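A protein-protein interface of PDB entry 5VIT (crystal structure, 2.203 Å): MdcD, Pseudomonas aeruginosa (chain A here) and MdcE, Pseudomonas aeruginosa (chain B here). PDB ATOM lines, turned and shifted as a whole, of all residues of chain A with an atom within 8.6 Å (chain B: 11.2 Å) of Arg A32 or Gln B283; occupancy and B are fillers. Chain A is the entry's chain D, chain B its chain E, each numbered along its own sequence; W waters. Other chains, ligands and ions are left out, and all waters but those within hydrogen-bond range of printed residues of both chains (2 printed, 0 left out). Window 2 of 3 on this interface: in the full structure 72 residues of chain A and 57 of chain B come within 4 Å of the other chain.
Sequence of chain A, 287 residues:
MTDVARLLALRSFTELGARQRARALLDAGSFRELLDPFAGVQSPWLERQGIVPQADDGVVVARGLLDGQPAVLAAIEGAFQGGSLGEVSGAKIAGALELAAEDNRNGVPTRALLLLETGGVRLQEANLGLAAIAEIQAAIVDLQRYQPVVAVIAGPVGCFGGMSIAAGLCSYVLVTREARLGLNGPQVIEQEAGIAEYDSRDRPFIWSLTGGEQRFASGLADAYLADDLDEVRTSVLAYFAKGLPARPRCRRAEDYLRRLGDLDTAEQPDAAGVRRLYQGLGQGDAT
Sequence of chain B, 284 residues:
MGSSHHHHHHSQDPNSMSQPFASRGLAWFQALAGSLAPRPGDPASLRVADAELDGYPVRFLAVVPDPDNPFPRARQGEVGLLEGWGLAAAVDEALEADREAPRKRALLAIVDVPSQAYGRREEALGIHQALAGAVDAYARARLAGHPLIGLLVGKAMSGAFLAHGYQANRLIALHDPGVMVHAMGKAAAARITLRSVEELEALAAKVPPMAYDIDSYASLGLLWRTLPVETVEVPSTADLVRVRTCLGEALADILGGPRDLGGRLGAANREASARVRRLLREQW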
ATOM      1  N   ALA A  22     -15.466  16.471 -17.253  1.00  0.00           N
ATOM      2  CA  ALA A  22     -14.599  15.917 -16.212  1.00  0.00           C
ATOM      3  C   ALA A  22     -15.336  14.869 -15.381  1.00  0.00           C
ATOM      4  O   ALA A  22     -14.768  13.826 -15.042  1.00  0.00           O
ATOM      5  CB  ALA A  22     -14.061  17.021 -15.321  1.00  0.00           C
ATOM      6  N   ARG A  23     -16.601  15.139 -15.060  1.00  0.00           N
ATOM      7  CA  ARG A  23     -17.380  14.188 -14.283  1.00  0.00           C
ATOM      8  C   ARG A  23     -17.650  12.920 -15.110  1.00  0.00           C
ATOM      9  O   ARG A  23     -17.653  11.810 -14.584  1.00  0.00           O
ATOM     10  CB  ARG A  23     -18.689  14.828 -13.803  1.00  0.00           C
ATOM     11  CG  ARG A  23     -19.469  13.980 -12.824  1.00  0.00           C
ATOM     12  CD  ARG A  23     -20.736  14.676 -12.334  1.00  0.00           C
ATOM     13  NE  ARG A  23     -20.500  15.433 -11.107  1.00  0.00           N
ATOM     14  CZ  ARG A  23     -20.492  16.759 -11.048  1.00  0.00           C
ATOM     15  NH1 ARG A  23     -20.732  17.469 -12.140  1.00  0.00           N
ATOM     16  NH2 ARG A  23     -20.264  17.375  -9.902  1.00  0.00           N
ATOM     17  N   LEU A  26     -14.039  10.590 -15.603  1.00  0.00           N
ATOM     18  CA  LEU A  26     -13.639   9.897 -14.373  1.00  0.00           C
ATOM     19  C   LEU A  26     -14.588   8.742 -14.037  1.00  0.00           C
ATOM     20  O   LEU A  26     -15.749   8.736 -14.473  1.00  0.00           O
ATOM     21  CB  LEU A  26     -13.580  10.882 -13.195  1.00  0.00           C
ATOM     22  CG  LEU A  26     -12.424  11.885 -13.285  1.00  0.00           C
ATOM     23  CD1 LEU A  26     -12.446  12.892 -12.136  1.00  0.00           C
ATOM     24  CD2 LEU A  26     -11.096  11.133 -13.336  1.00  0.00           C
ATOM     25  N   ASP A  27     -14.094   7.766 -13.273  1.00  0.00           N
ATOM     26  CA  ASP A  27     -14.923   6.635 -12.866  1.00  0.00           C
ATOM     27  C   ASP A  27     -16.171   7.138 -12.154  1.00  0.00           C
ATOM     28  O   ASP A  27     -16.085   8.024 -11.303  1.00  0.00           O
ATOM     29  CB  ASP A  27     -14.170   5.680 -11.935  1.00  0.00           C
ATOM     30  CG  ASP A  27     -13.097   4.876 -12.638  1.00  0.00           C
ATOM     31  OD1 ASP A  27     -12.987   4.947 -13.881  1.00  0.00           O
ATOM     32  OD2 ASP A  27     -12.364   4.158 -11.922  1.00  0.00           O
ATOM     33  N   GLY A  29     -18.853   8.079  -9.767  1.00  0.00           N
ATOM     34  CA  GLY A  29     -18.738   8.227  -8.331  1.00  0.00           C
ATOM     35  C   GLY A  29     -17.432   8.810  -7.810  1.00  0.00           C
ATOM     36  O   GLY A  29     -17.404   9.324  -6.696  1.00  0.00           O
ATOM     37  N   SER A  30     -16.352   8.752  -8.589  1.00  0.00           N
ATOM     38  CA  SER A  30     -15.051   9.135  -8.040  1.00  0.00           C
ATOM     39  C   SER A  30     -14.777  10.640  -8.100  1.00  0.00           C
ATOM     40  O   SER A  30     -13.877  11.116  -7.420  1.00  0.00           O
ATOM     41  CB  SER A  30     -13.913   8.389  -8.744  1.00  0.00           C
ATOM     42  OG  SER A  30     -13.685   8.892 -10.053  1.00  0.00           O
ATOM     43  N   PHE A  31     -15.556  11.381  -8.883  1.00  0.00           N
ATOM     44  CA  PHE A  31     -15.308  12.813  -9.110  1.00  0.00           C
ATOM     45  C   PHE A  31     -15.254  13.644  -7.823  1.00  0.00           C
ATOM     46  O   PHE A  31     -16.214  13.672  -7.052  1.00  0.00           O
ATOM     47  CB  PHE A  31     -16.377  13.379 -10.047  1.00  0.00           C
ATOM     48  CG  PHE A  31     -16.256  14.856 -10.301  1.00  0.00           C
ATOM     49  CD1 PHE A  31     -15.536  15.329 -11.388  1.00  0.00           C
ATOM     50  CD2 PHE A  31     -16.892  15.770  -9.477  1.00  0.00           C
ATOM     51  CE1 PHE A  31     -15.430  16.675 -11.631  1.00  0.00           C
ATOM     52  CE2 PHE A  31     -16.790  17.127  -9.711  1.00  0.00           C
ATOM     53  CZ  PHE A  31     -16.058  17.583 -10.782  1.00  0.00           C
ATOM     54  N   ARG A  32     -14.130  14.326  -7.590  1.00  0.00           N
ATOM     55  CA  ARG A  32     -14.021  15.210  -6.424  1.00  0.00           C
ATOM     56  C   ARG A  32     -13.217  16.462  -6.762  1.00  0.00           C
ATOM     57  O   ARG A  32     -12.009  16.397  -6.978  1.00  0.00           O
ATOM     58  CB  ARG A  32     -13.386  14.477  -5.229  1.00  0.00           C
ATOM     59  CG  ARG A  32     -13.515  15.251  -3.919  1.00  0.00           C
ATOM     60  CD  ARG A  32     -12.895  14.515  -2.740  1.00  0.00           C
ATOM     61  NE  ARG A  32     -11.490  14.862  -2.572  1.00  0.00           N
ATOM     62  CZ  ARG A  32     -10.493  14.086  -2.968  1.00  0.00           C
ATOM     63  NH1 ARG A  32     -10.767  12.917  -3.540  1.00  0.00           N
ATOM     64  NH2 ARG A  32      -9.237  14.473  -2.791  1.00  0.00           N
ATOM     65  N   GLU A  33     -13.891  17.604  -6.806  1.00  0.00           N
ATOM     66  CA  GLU A  33     -13.272  18.816  -7.328  1.00  0.00           C
ATOM     67  C   GLU A  33     -12.408  19.516  -6.281  1.00  0.00           C
ATOM     68  O   GLU A  33     -12.786  19.647  -5.122  1.00  0.00           O
ATOM     69  CB  GLU A  33     -14.349  19.789  -7.863  1.00  0.00           C
ATOM     70  CG  GLU A  33     -13.792  21.005  -8.637  1.00  0.00           C
ATOM     71  CD  GLU A  33     -14.867  21.802  -9.400  1.00  0.00           C
ATOM     72  OE1 GLU A  33     -15.995  21.303  -9.581  1.00  0.00           O
ATOM     73  OE2 GLU A  33     -14.580  22.943  -9.811  1.00  0.00           O
ATOM     74  N   LEU A  34     -11.247  19.984  -6.716  1.00  0.00           N
ATOM     75  CA  LEU A  34     -10.389  20.798  -5.866  1.00  0.00           C
ATOM     76  C   LEU A  34     -10.557  22.254  -6.253  1.00  0.00           C
ATOM     77  O   LEU A  34     -10.603  22.576  -7.444  1.00  0.00           O
ATOM     78  CB  LEU A  34      -8.917  20.382  -6.004  1.00  0.00           C
ATOM     79  CG  LEU A  34      -8.643  18.879  -5.909  1.00  0.00           C
ATOM     80  CD1 LEU A  34      -7.167  18.568  -6.047  1.00  0.00           C
ATOM     81  CD2 LEU A  34      -9.205  18.306  -4.619  1.00  0.00           C
ATOM     82  N   LEU A  35     -10.621  23.124  -5.253  1.00  0.00           N
ATOM     83  CA  LEU A  35     -10.768  24.557  -5.472  1.00  0.00           C
ATOM     84  C   LEU A  35     -12.014  24.811  -6.312  1.00  0.00           C
ATOM     85  O   LEU A  35     -11.971  25.511  -7.324  1.00  0.00           O
ATOM     86  CB  LEU A  35      -9.508  25.138  -6.131  1.00  0.00           C
ATOM     87  CG  LEU A  35      -8.317  25.370  -5.189  1.00  0.00           C
ATOM     88  CD1 LEU A  35      -7.715  24.075  -4.653  1.00  0.00           C
ATOM     89  CD2 LEU A  35      -7.237  26.236  -5.837  1.00  0.00           C
ATOM     90  N   ASP A  36     -13.119  24.214  -5.879  1.00  0.00           N
ATOM     91  CA  ASP A  36     -14.381  24.298  -6.598  1.00  0.00           C
ATOM     92  C   ASP A  36     -14.940  25.719  -6.484  1.00  0.00           C
ATOM     93  O   ASP A  36     -14.424  26.527  -5.703  1.00  0.00           O
ATOM     94  CB  ASP A  36     -15.385  23.220  -6.089  1.00  0.00           C
ATOM     95  CG  ASP A  36     -15.894  23.460  -4.662  1.00  0.00           C
ATOM     96  OD1 ASP A  36     -16.299  22.455  -4.041  1.00  0.00           O
ATOM     97  OD2 ASP A  36     -15.925  24.609  -4.160  1.00  0.00           O
ATOM     98  N   ALA A  39     -15.136  27.692  -3.199  1.00  0.00           N
ATOM     99  CA  ALA A  39     -13.892  28.143  -2.572  1.00  0.00           C
ATOM    100  C   ALA A  39     -13.601  29.611  -2.922  1.00  0.00           C
ATOM    101  O   ALA A  39     -12.759  30.239  -2.306  1.00  0.00           O
ATOM    102  CB  ALA A  39     -12.725  27.253  -2.991  1.00  0.00           C
ATOM    103  N   VAL A  41     -11.899  30.986  -5.201  1.00  0.00           N
ATOM    104  CA  VAL A  41     -10.529  31.279  -5.651  1.00  0.00           C
ATOM    105  C   VAL A  41     -10.536  31.678  -7.122  1.00  0.00           C
ATOM    106  O   VAL A  41     -10.326  30.841  -7.995  1.00  0.00           O
ATOM    107  CB  VAL A  41      -9.579  30.076  -5.459  1.00  0.00           C
ATOM    108  CG1 VAL A  41      -8.118  30.485  -5.794  1.00  0.00           C
ATOM    109  CG2 VAL A  41      -9.670  29.554  -4.028  1.00  0.00           C
ATOM    110  N   VAL A  60     -11.597  23.445 -14.258  1.00  0.00           N
ATOM    111  CA  VAL A  60     -12.063  22.449 -13.307  1.00  0.00           C
ATOM    112  C   VAL A  60     -10.928  21.475 -12.989  1.00  0.00           C
ATOM    113  O   VAL A  60     -10.421  20.801 -13.898  1.00  0.00           O
ATOM    114  CB  VAL A  60     -13.268  21.648 -13.874  1.00  0.00           C
ATOM    115  CG1 VAL A  60     -13.803  20.647 -12.837  1.00  0.00           C
ATOM    116  CG2 VAL A  60     -14.362  22.586 -14.360  1.00  0.00           C
ATOM    117  N   VAL A  61     -10.512  21.405 -11.726  1.00  0.00           N
ATOM    118  CA  VAL A  61      -9.537  20.384 -11.321  1.00  0.00           C
ATOM    119  C   VAL A  61     -10.205  19.374 -10.399  1.00  0.00           C
ATOM    120  O   VAL A  61     -10.759  19.738  -9.369  1.00  0.00           O
ATOM    121  CB  VAL A  61      -8.322  20.989 -10.613  1.00  0.00           C
ATOM    122  CG1 VAL A  61      -7.492  19.888  -9.962  1.00  0.00           C
ATOM    123  CG2 VAL A  61      -7.493  21.773 -11.602  1.00  0.00           C
ATOM    124  N   ALA A  62     -10.187  18.103 -10.791  1.00  0.00           N
ATOM    125  CA  ALA A  62     -10.822  17.078  -9.973  1.00  0.00           C
ATOM    126  C   ALA A  62      -9.900  15.895  -9.772  1.00  0.00           C
ATOM    127  O   ALA A  62      -9.148  15.497 -10.676  1.00  0.00           O
ATOM    128  CB  ALA A  62     -12.132  16.624 -10.595  1.00  0.00           C
ATOM    129  N   ARG A  63      -9.945  15.363  -8.556  1.00  0.00           N
ATOM    130  CA  ARG A  63      -9.366  14.070  -8.258  1.00  0.00           C
ATOM    131  C   ARG A  63     -10.416  13.018  -8.589  1.00  0.00           C
ATOM    132  O   ARG A  63     -11.611  13.320  -8.676  1.00  0.00           O
ATOM    133  CB  ARG A  63      -8.958  13.973  -6.789  1.00  0.00           C
ATOM    134  CG  ARG A  63      -7.963  15.013  -6.327  1.00  0.00           C
ATOM    135  CD  ARG A  63      -6.615  14.833  -6.971  1.00  0.00           C
ATOM    136  NE  ARG A  63      -6.260  13.428  -7.140  1.00  0.00           N
ATOM    137  CZ  ARG A  63      -5.849  12.632  -6.158  1.00  0.00           C
ATOM    138  NH1 ARG A  63      -5.753  13.088  -4.921  1.00  0.00           N
ATOM    139  NH2 ARG A  63      -5.540  11.374  -6.419  1.00  0.00           N
ATOM    140  N   GLY A  64      -9.982  11.781  -8.759  1.00  0.00           N
ATOM    141  CA  GLY A  64     -10.913  10.689  -8.938  1.00  0.00           C
ATOM    142  C   GLY A  64     -10.149   9.437  -9.299  1.00  0.00           C
ATOM    143  O   GLY A  64      -8.948   9.312  -8.998  1.00  0.00           O
ATOM    144  N   LEU A  65     -10.852   8.511  -9.944  1.00  0.00           N
ATOM    145  CA  LEU A  65     -10.254   7.284 -10.430  1.00  0.00           C
ATOM    146  C   LEU A  65     -10.403   7.156 -11.943  1.00  0.00           C
ATOM    147  O   LEU A  65     -11.425   7.542 -12.517  1.00  0.00           O
ATOM    148  CB  LEU A  65     -10.884   6.080  -9.731  1.00  0.00           C
ATOM    149  CG  LEU A  65     -10.808   6.092  -8.202  1.00  0.00           C
ATOM    150  CD1 LEU A  65     -11.564   4.903  -7.646  1.00  0.00           C
ATOM    151  CD2 LEU A  65      -9.357   6.107  -7.697  1.00  0.00           C
ATOM    152  N   ALA A  71      -6.160   9.327  -9.974  1.00  0.00           N
ATOM    153  CA  ALA A  71      -6.072  10.268 -11.081  1.00  0.00           C
ATOM    154  C   ALA A  71      -6.417  11.708 -10.700  1.00  0.00           C
ATOM    155  O   ALA A  71      -7.099  11.985  -9.715  1.00  0.00           O
ATOM    156  CB  ALA A  71      -6.970   9.808 -12.215  1.00  0.00           C
ATOM    157  N   VAL A  72      -5.922  12.622 -11.511  1.00  0.00           N
ATOM    158  CA  VAL A  72      -6.302  14.010 -11.422  1.00  0.00           C
ATOM    159  C   VAL A  72      -6.639  14.445 -12.845  1.00  0.00           C
ATOM    160  O   VAL A  72      -6.017  13.993 -13.815  1.00  0.00           O
ATOM    161  CB  VAL A  72      -5.184  14.889 -10.798  1.00  0.00           C
ATOM    162  CG1 VAL A  72      -3.955  14.941 -11.700  1.00  0.00           C
ATOM    163  CG2 VAL A  72      -5.705  16.281 -10.505  1.00  0.00           C
ATOM    164  N   LEU A  73      -7.647  15.296 -12.964  1.00  0.00           N
ATOM    165  CA  LEU A  73      -8.126  15.739 -14.259  1.00  0.00           C
ATOM    166  C   LEU A  73      -8.229  17.268 -14.244  1.00  0.00           C
ATOM    167  O   LEU A  73      -8.885  17.822 -13.379  1.00  0.00           O
ATOM    168  CB  LEU A  73      -9.474  15.079 -14.554  1.00  0.00           C
ATOM    169  CG  LEU A  73     -10.119  15.153 -15.945  1.00  0.00           C
ATOM    170  CD1 LEU A  73     -11.270  14.163 -16.021  1.00  0.00           C
ATOM    171  CD2 LEU A  73     -10.601  16.551 -16.276  1.00  0.00           C
ATOM    172  N   LYS A  92      -3.758  26.294 -10.984  1.00  0.00           N
ATOM    173  CA  LYS A  92      -4.548  25.095 -10.712  1.00  0.00           C
ATOM    174  C   LYS A  92      -4.049  23.907 -11.559  1.00  0.00           C
ATOM    175  O   LYS A  92      -3.873  22.801 -11.037  1.00  0.00           O
ATOM    176  CB  LYS A  92      -6.044  25.339 -10.969  1.00  0.00           C
ATOM    177  CG  LYS A  92      -6.743  26.272  -9.962  1.00  0.00           C
ATOM    178  CD  LYS A  92      -8.229  26.560 -10.350  1.00  0.00           C
ATOM    179  CE  LYS A  92      -9.180  25.420  -9.950  1.00  0.00           C
ATOM    180  NZ  LYS A  92     -10.672  25.778  -9.943  1.00  0.00           N
ATOM    181  N   LEU A  99       1.586  17.826  -8.056  1.00  0.00           N
ATOM    182  CA  LEU A  99       1.262  16.904  -6.968  1.00  0.00           C
ATOM    183  C   LEU A  99       1.205  15.469  -7.484  1.00  0.00           C
ATOM    184  O   LEU A  99       1.530  14.529  -6.762  1.00  0.00           O
ATOM    185  CB  LEU A  99      -0.055  17.296  -6.279  1.00  0.00           C
ATOM    186  CG  LEU A  99       0.132  18.557  -5.418  1.00  0.00           C
ATOM    187  CD1 LEU A  99      -1.177  19.181  -5.008  1.00  0.00           C
ATOM    188  CD2 LEU A  99       0.992  18.268  -4.176  1.00  0.00           C
ATOM    189  N   ALA B 274       0.883  30.939  -5.317  1.00  0.00           N
ATOM    190  CA  ALA B 274       1.329  30.220  -4.125  1.00  0.00           C
ATOM    191  C   ALA B 274       0.128  29.677  -3.340  1.00  0.00           C
ATOM    192  O   ALA B 274       0.140  28.534  -2.878  1.00  0.00           O
ATOM    193  CB  ALA B 274       2.193  31.134  -3.238  1.00  0.00           C
ATOM    194  N   ARG B 275      -0.917  30.491  -3.215  1.00  0.00           N
ATOM    195  CA  ARG B 275      -2.095  30.079  -2.455  1.00  0.00           C
ATOM    196  C   ARG B 275      -2.774  28.886  -3.124  1.00  0.00           C
ATOM    197  O   ARG B 275      -3.168  27.943  -2.452  1.00  0.00           O
ATOM    198  CB  ARG B 275      -3.089  31.235  -2.287  1.00  0.00           C
ATOM    199  CG  ARG B 275      -4.328  30.865  -1.450  1.00  0.00           C
ATOM    200  CD  ARG B 275      -5.048  32.114  -0.995  1.00  0.00           C
ATOM    201  NE  ARG B 275      -4.999  33.129  -2.049  1.00  0.00           N
ATOM    202  CZ  ARG B 275      -6.032  33.459  -2.816  1.00  0.00           C
ATOM    203  NH1 ARG B 275      -7.211  32.871  -2.628  1.00  0.00           N
ATOM    204  NH2 ARG B 275      -5.898  34.390  -3.745  1.00  0.00           N
ATOM    205  N   VAL B 276      -2.883  28.916  -4.442  1.00  0.00           N
ATOM    206  CA  VAL B 276      -3.504  27.802  -5.141  1.00  0.00           C
ATOM    207  C   VAL B 276      -2.785  26.480  -4.819  1.00  0.00           C
ATOM    208  O   VAL B 276      -3.430  25.478  -4.519  1.00  0.00           O
ATOM    209  CB  VAL B 276      -3.536  28.037  -6.672  1.00  0.00           C
ATOM    210  CG1 VAL B 276      -3.797  26.727  -7.424  1.00  0.00           C
ATOM    211  CG2 VAL B 276      -4.602  29.075  -7.006  1.00  0.00           C
ATOM    212  N   ARG B 277      -1.454  26.487  -4.850  1.00  0.00           N
ATOM    213  CA  ARG B 277      -0.691  25.261  -4.570  1.00  0.00           C
ATOM    214  C   ARG B 277      -0.877  24.777  -3.129  1.00  0.00           C
ATOM    215  O   ARG B 277      -0.959  23.576  -2.874  1.00  0.00           O
ATOM    216  CB  ARG B 277       0.794  25.485  -4.874  1.00  0.00           C
ATOM    217  CG  ARG B 277       1.071  25.559  -6.375  1.00  0.00           C
ATOM    218  CD  ARG B 277       2.486  25.971  -6.648  1.00  0.00           C
ATOM    219  NE  ARG B 277       2.873  25.687  -8.027  1.00  0.00           N
ATOM    220  CZ  ARG B 277       2.585  26.471  -9.060  1.00  0.00           C
ATOM    221  NH1 ARG B 277       1.917  27.611  -8.869  1.00  0.00           N
ATOM    222  NH2 ARG B 277       2.989  26.125 -10.277  1.00  0.00           N
ATOM    223  N   ARG B 278      -0.945  25.722  -2.201  1.00  0.00           N
ATOM    224  CA  ARG B 278      -1.220  25.412  -0.801  1.00  0.00           C
ATOM    225  C   ARG B 278      -2.591  24.750  -0.664  1.00  0.00           C
ATOM    226  O   ARG B 278      -2.761  23.744   0.032  1.00  0.00           O
ATOM    227  CB  ARG B 278      -1.148  26.693   0.039  1.00  0.00           C
ATOM    228  CG  ARG B 278      -0.991  26.471   1.522  1.00  0.00           C
ATOM    229  CD  ARG B 278      -0.867  27.816   2.266  1.00  0.00           C
ATOM    230  NE  ARG B 278      -1.975  28.756   2.008  1.00  0.00           N
ATOM    231  CZ  ARG B 278      -3.231  28.613   2.456  1.00  0.00           C
ATOM    232  NH1 ARG B 278      -3.577  27.544   3.165  1.00  0.00           N
ATOM    233  NH2 ARG B 278      -4.162  29.532   2.182  1.00  0.00           N
ATOM    234  N   LEU B 279      -3.572  25.309  -1.357  1.00  0.00           N
ATOM    235  CA  LEU B 279      -4.929  24.815  -1.232  1.00  0.00           C
ATOM    236  C   LEU B 279      -5.038  23.453  -1.912  1.00  0.00           C
ATOM    237  O   LEU B 279      -5.732  22.558  -1.421  1.00  0.00           O
ATOM    238  CB  LEU B 279      -5.908  25.815  -1.823  1.00  0.00           C
ATOM    239  CG  LEU B 279      -6.109  27.096  -1.023  1.00  0.00           C
ATOM    240  CD1 LEU B 279      -6.958  28.099  -1.824  1.00  0.00           C
ATOM    241  CD2 LEU B 279      -6.738  26.809   0.365  1.00  0.00           C
ATOM    242  N   LEU B 280      -4.316  23.282  -3.018  1.00  0.00           N
ATOM    243  CA  LEU B 280      -4.306  21.997  -3.700  1.00  0.00           C
ATOM    244  C   LEU B 280      -3.769  20.872  -2.809  1.00  0.00           C
ATOM    245  O   LEU B 280      -4.357  19.785  -2.793  1.00  0.00           O
ATOM    246  CB  LEU B 280      -3.501  22.080  -4.986  1.00  0.00           C
ATOM    247  CG  LEU B 280      -4.188  22.756  -6.180  1.00  0.00           C
ATOM    248  CD1 LEU B 280      -3.206  22.920  -7.364  1.00  0.00           C
ATOM    249  CD2 LEU B 280      -5.406  21.951  -6.579  1.00  0.00           C
ATOM    250  N   ARG B 281      -2.678  21.100  -2.068  1.00  0.00           N
ATOM    251  CA  ARG B 281      -2.169  20.001  -1.241  1.00  0.00           C
ATOM    252  C   ARG B 281      -3.076  19.729  -0.049  1.00  0.00           C
ATOM    253  O   ARG B 281      -3.198  18.587   0.354  1.00  0.00           O
ATOM    254  CB  ARG B 281      -0.750  20.226  -0.723  1.00  0.00           C
ATOM    255  CG  ARG B 281      -0.152  18.874  -0.257  1.00  0.00           C
ATOM    256  CD  ARG B 281       1.105  19.042   0.535  1.00  0.00           C
ATOM    257  NE  ARG B 281       2.172  18.170   0.059  1.00  0.00           N
ATOM    258  CZ  ARG B 281       2.947  18.550  -0.959  1.00  0.00           C
ATOM    259  NH1 ARG B 281       2.693  19.731  -1.537  1.00  0.00           N
ATOM    260  NH2 ARG B 281       3.945  17.790  -1.436  1.00  0.00           N
ATOM    261  N   GLU B 282      -3.693  20.761   0.519  1.00  0.00           N
ATOM    262  CA  GLU B 282      -4.599  20.563   1.648  1.00  0.00           C
ATOM    263  C   GLU B 282      -5.724  19.619   1.252  1.00  0.00           C
ATOM    264  O   GLU B 282      -6.171  18.808   2.054  1.00  0.00           O
ATOM    265  CB  GLU B 282      -5.210  21.888   2.126  1.00  0.00           C
ATOM    266  CG  GLU B 282      -4.284  22.813   2.899  1.00  0.00           C
ATOM    267  CD  GLU B 282      -4.951  24.145   3.243  1.00  0.00           C
ATOM    268  OE1 GLU B 282      -6.155  24.314   2.943  1.00  0.00           O
ATOM    269  OE2 GLU B 282      -4.277  25.025   3.816  1.00  0.00           O
ATOM    270  N   GLN B 283      -6.171  19.721   0.006  1.00  0.00           N
ATOM    271  CA  GLN B 283      -7.363  19.003  -0.444  1.00  0.00           C
ATOM    272  C   GLN B 283      -7.040  17.743  -1.237  1.00  0.00           C
ATOM    273  O   GLN B 283      -7.940  16.989  -1.598  1.00  0.00           O
ATOM    274  CB  GLN B 283      -8.249  19.942  -1.293  1.00  0.00           C
ATOM    275  CG  GLN B 283      -8.745  21.170  -0.521  1.00  0.00           C
ATOM    276  CD  GLN B 283      -9.267  22.303  -1.408  1.00  0.00           C
ATOM    277  OE1 GLN B 283      -9.962  22.088  -2.419  1.00  0.00           O
ATOM    278  NE2 GLN B 283      -8.923  23.522  -1.031  1.00  0.00           N
ATOM    279  N   TRP B 284      -5.756  17.512  -1.499  1.00  0.00           N
ATOM    280  CA  TRP B 284      -5.340  16.489  -2.461  1.00  0.00           C
ATOM    281  C   TRP B 284      -5.751  15.087  -2.062  1.00  0.00           C
ATOM    282  O   TRP B 284      -6.265  14.324  -2.889  1.00  0.00           O
ATOM    283  CB  TRP B 284      -3.822  16.520  -2.653  1.00  0.00           C
ATOM    284  CG  TRP B 284      -3.306  15.683  -3.816  1.00  0.00           C
ATOM    285  CD1 TRP B 284      -2.652  14.474  -3.748  1.00  0.00           C
ATOM    286  CD2 TRP B 284      -3.393  16.008  -5.213  1.00  0.00           C
ATOM    287  NE1 TRP B 284      -2.320  14.035  -5.019  1.00  0.00           N
ATOM    288  CE2 TRP B 284      -2.765  14.957  -5.933  1.00  0.00           C
ATOM    289  CE3 TRP B 284      -3.930  17.085  -5.926  1.00  0.00           C
ATOM    290  CZ2 TRP B 284      -2.662  14.965  -7.327  1.00  0.00           C
ATOM    291  CZ3 TRP B 284      -3.828  17.086  -7.313  1.00  0.00           C
ATOM    292  CH2 TRP B 284      -3.204  16.030  -7.995  1.00  0.00           C
ATOM    293  OXT TRP B 284      -5.543  14.692  -0.915  1.00  0.00           O
HETATM  294  O   HOH W   1     -11.955  20.232  -2.508  1.00  0.00           O
HETATM  295  O   HOH W   2     -12.766  23.316  -2.932  1.00  0.00           O
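Arg A32 touches just these residues of chain B: Gln B283 and Trp B284.
Of chain A, only Arg A32 (3.1 Å), Leu A34 (3.5 Å) and Leu A35 (3.1 Å) come within 4 Å of Gln B283.
Phe A31 touches none of the printed residues of chain B.
Leu A34 touches just these residues of chain B: Leu B280, Gln B283 and Trp B284.
No residue of chain B comes within 4 Å of Ala A62.
Of the printed residues of chain B, Val A72 touches Trp B284 (3.6 Å).
Of the printed residues of chain A, Val B276 touches Leu A35, Val A41 and Lys A92.
Gly A29 touches none of the printed residues of chain B.
The nearest printed residue of chain B that does not touch Arg A32 is Glu B282 (7.2 Å).
The nearest printed residue of chain B that does not touch Leu A99 is Arg B277 (4.9 Å).
The guanidinium group (NH2) of Arg A32 is in hydrogen-bond range of the backbone carbonyl oxygen (O) of Gln B283 (3.1 Å).
The guanidinium group of Arg A32 is in salt-bridge range of the chain-end carboxylate of Trp B284 (3.0 Å).
The backbone NH of Leu A35 is in hydrogen-bond range of the side-chain amide oxygen of Gln B283, 3.1 Å away.
The guanidinium group (NH1) of Arg A63 lies within salt-bridge range of the chain-end carboxylate (O) of Trp B284.
Among the printed residues, pairs that only touch across the chains: Leu A99 with Arg B281 (3.5 Å), Leu A34 with Gln B283 (3.5 Å), Val A72 with Trp B284 (3.6 Å), Leu A34 with Trp B284 (3.6 Å), Leu A99 with Trp B284 (3.6 Å), Lys A92 with Val B276 (3.6 Å), Leu A35 with Leu B280 (3.7 Å), Leu A99 with Leu B280 (3.7 Å), Lys A92 with Leu B280 (3.7 Å), Leu A35 with Leu B279 (3.8 Å), Val A41 with Leu B279 (3.8 Å), Leu A35 with Val B276 (3.8 Å), Leu A34 with Leu B280 (3.9 Å) and Val A41 with Val B276 (3.98 Å).
Hydrophobic or aromatic side chains of chain A that line the printed part of chain B: Leu A34, Leu A35, Val A41, Val A72 and Leu A99.
Printed residues of chain B that touch a printed residue of chain A: Val B276, Leu B279, Leu B280, Arg B281, Gln B283 and Trp B284.
Hydrophobic or aromatic side chains of chain B that line the printed part of chain A: Val B276, Leu B279, Leu B280 and Trp B284.
Along chain B the printed residues that touch a printed residue of chain A span positions 276 to 284.
Among the printed residues, no Asp or Glu carboxylate lies within 4 Å of a Lys or Arg side-chain nitrogen of the other chain.
Water W1 lies within hydrogen-bond range of the side-chain amide oxygen (OE1) of Gln B283 (2.7 Å) and the backbone carbonyl oxygen (O) of Glu A33 (2.8 Å).
Water W2 lies within hydrogen-bond range of the backbone NH (N) of Asp A36, the side-chain amide oxygen (OE1) of Gln B283 and the backbone NH (N) of Leu A35.
O of Arg A32 lies within hydrogen-bond range of N of Arg A63.
O of Leu A35 is in hydrogen-bond range of NZ of Lys A92 (2.9 Å).
O of Ala A71 sits at hydrogen-bond distance from NE of Arg A63, at 3.1 Å.
O of Leu B279 is in hydrogen-bond range of NE2 of Gln B283.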
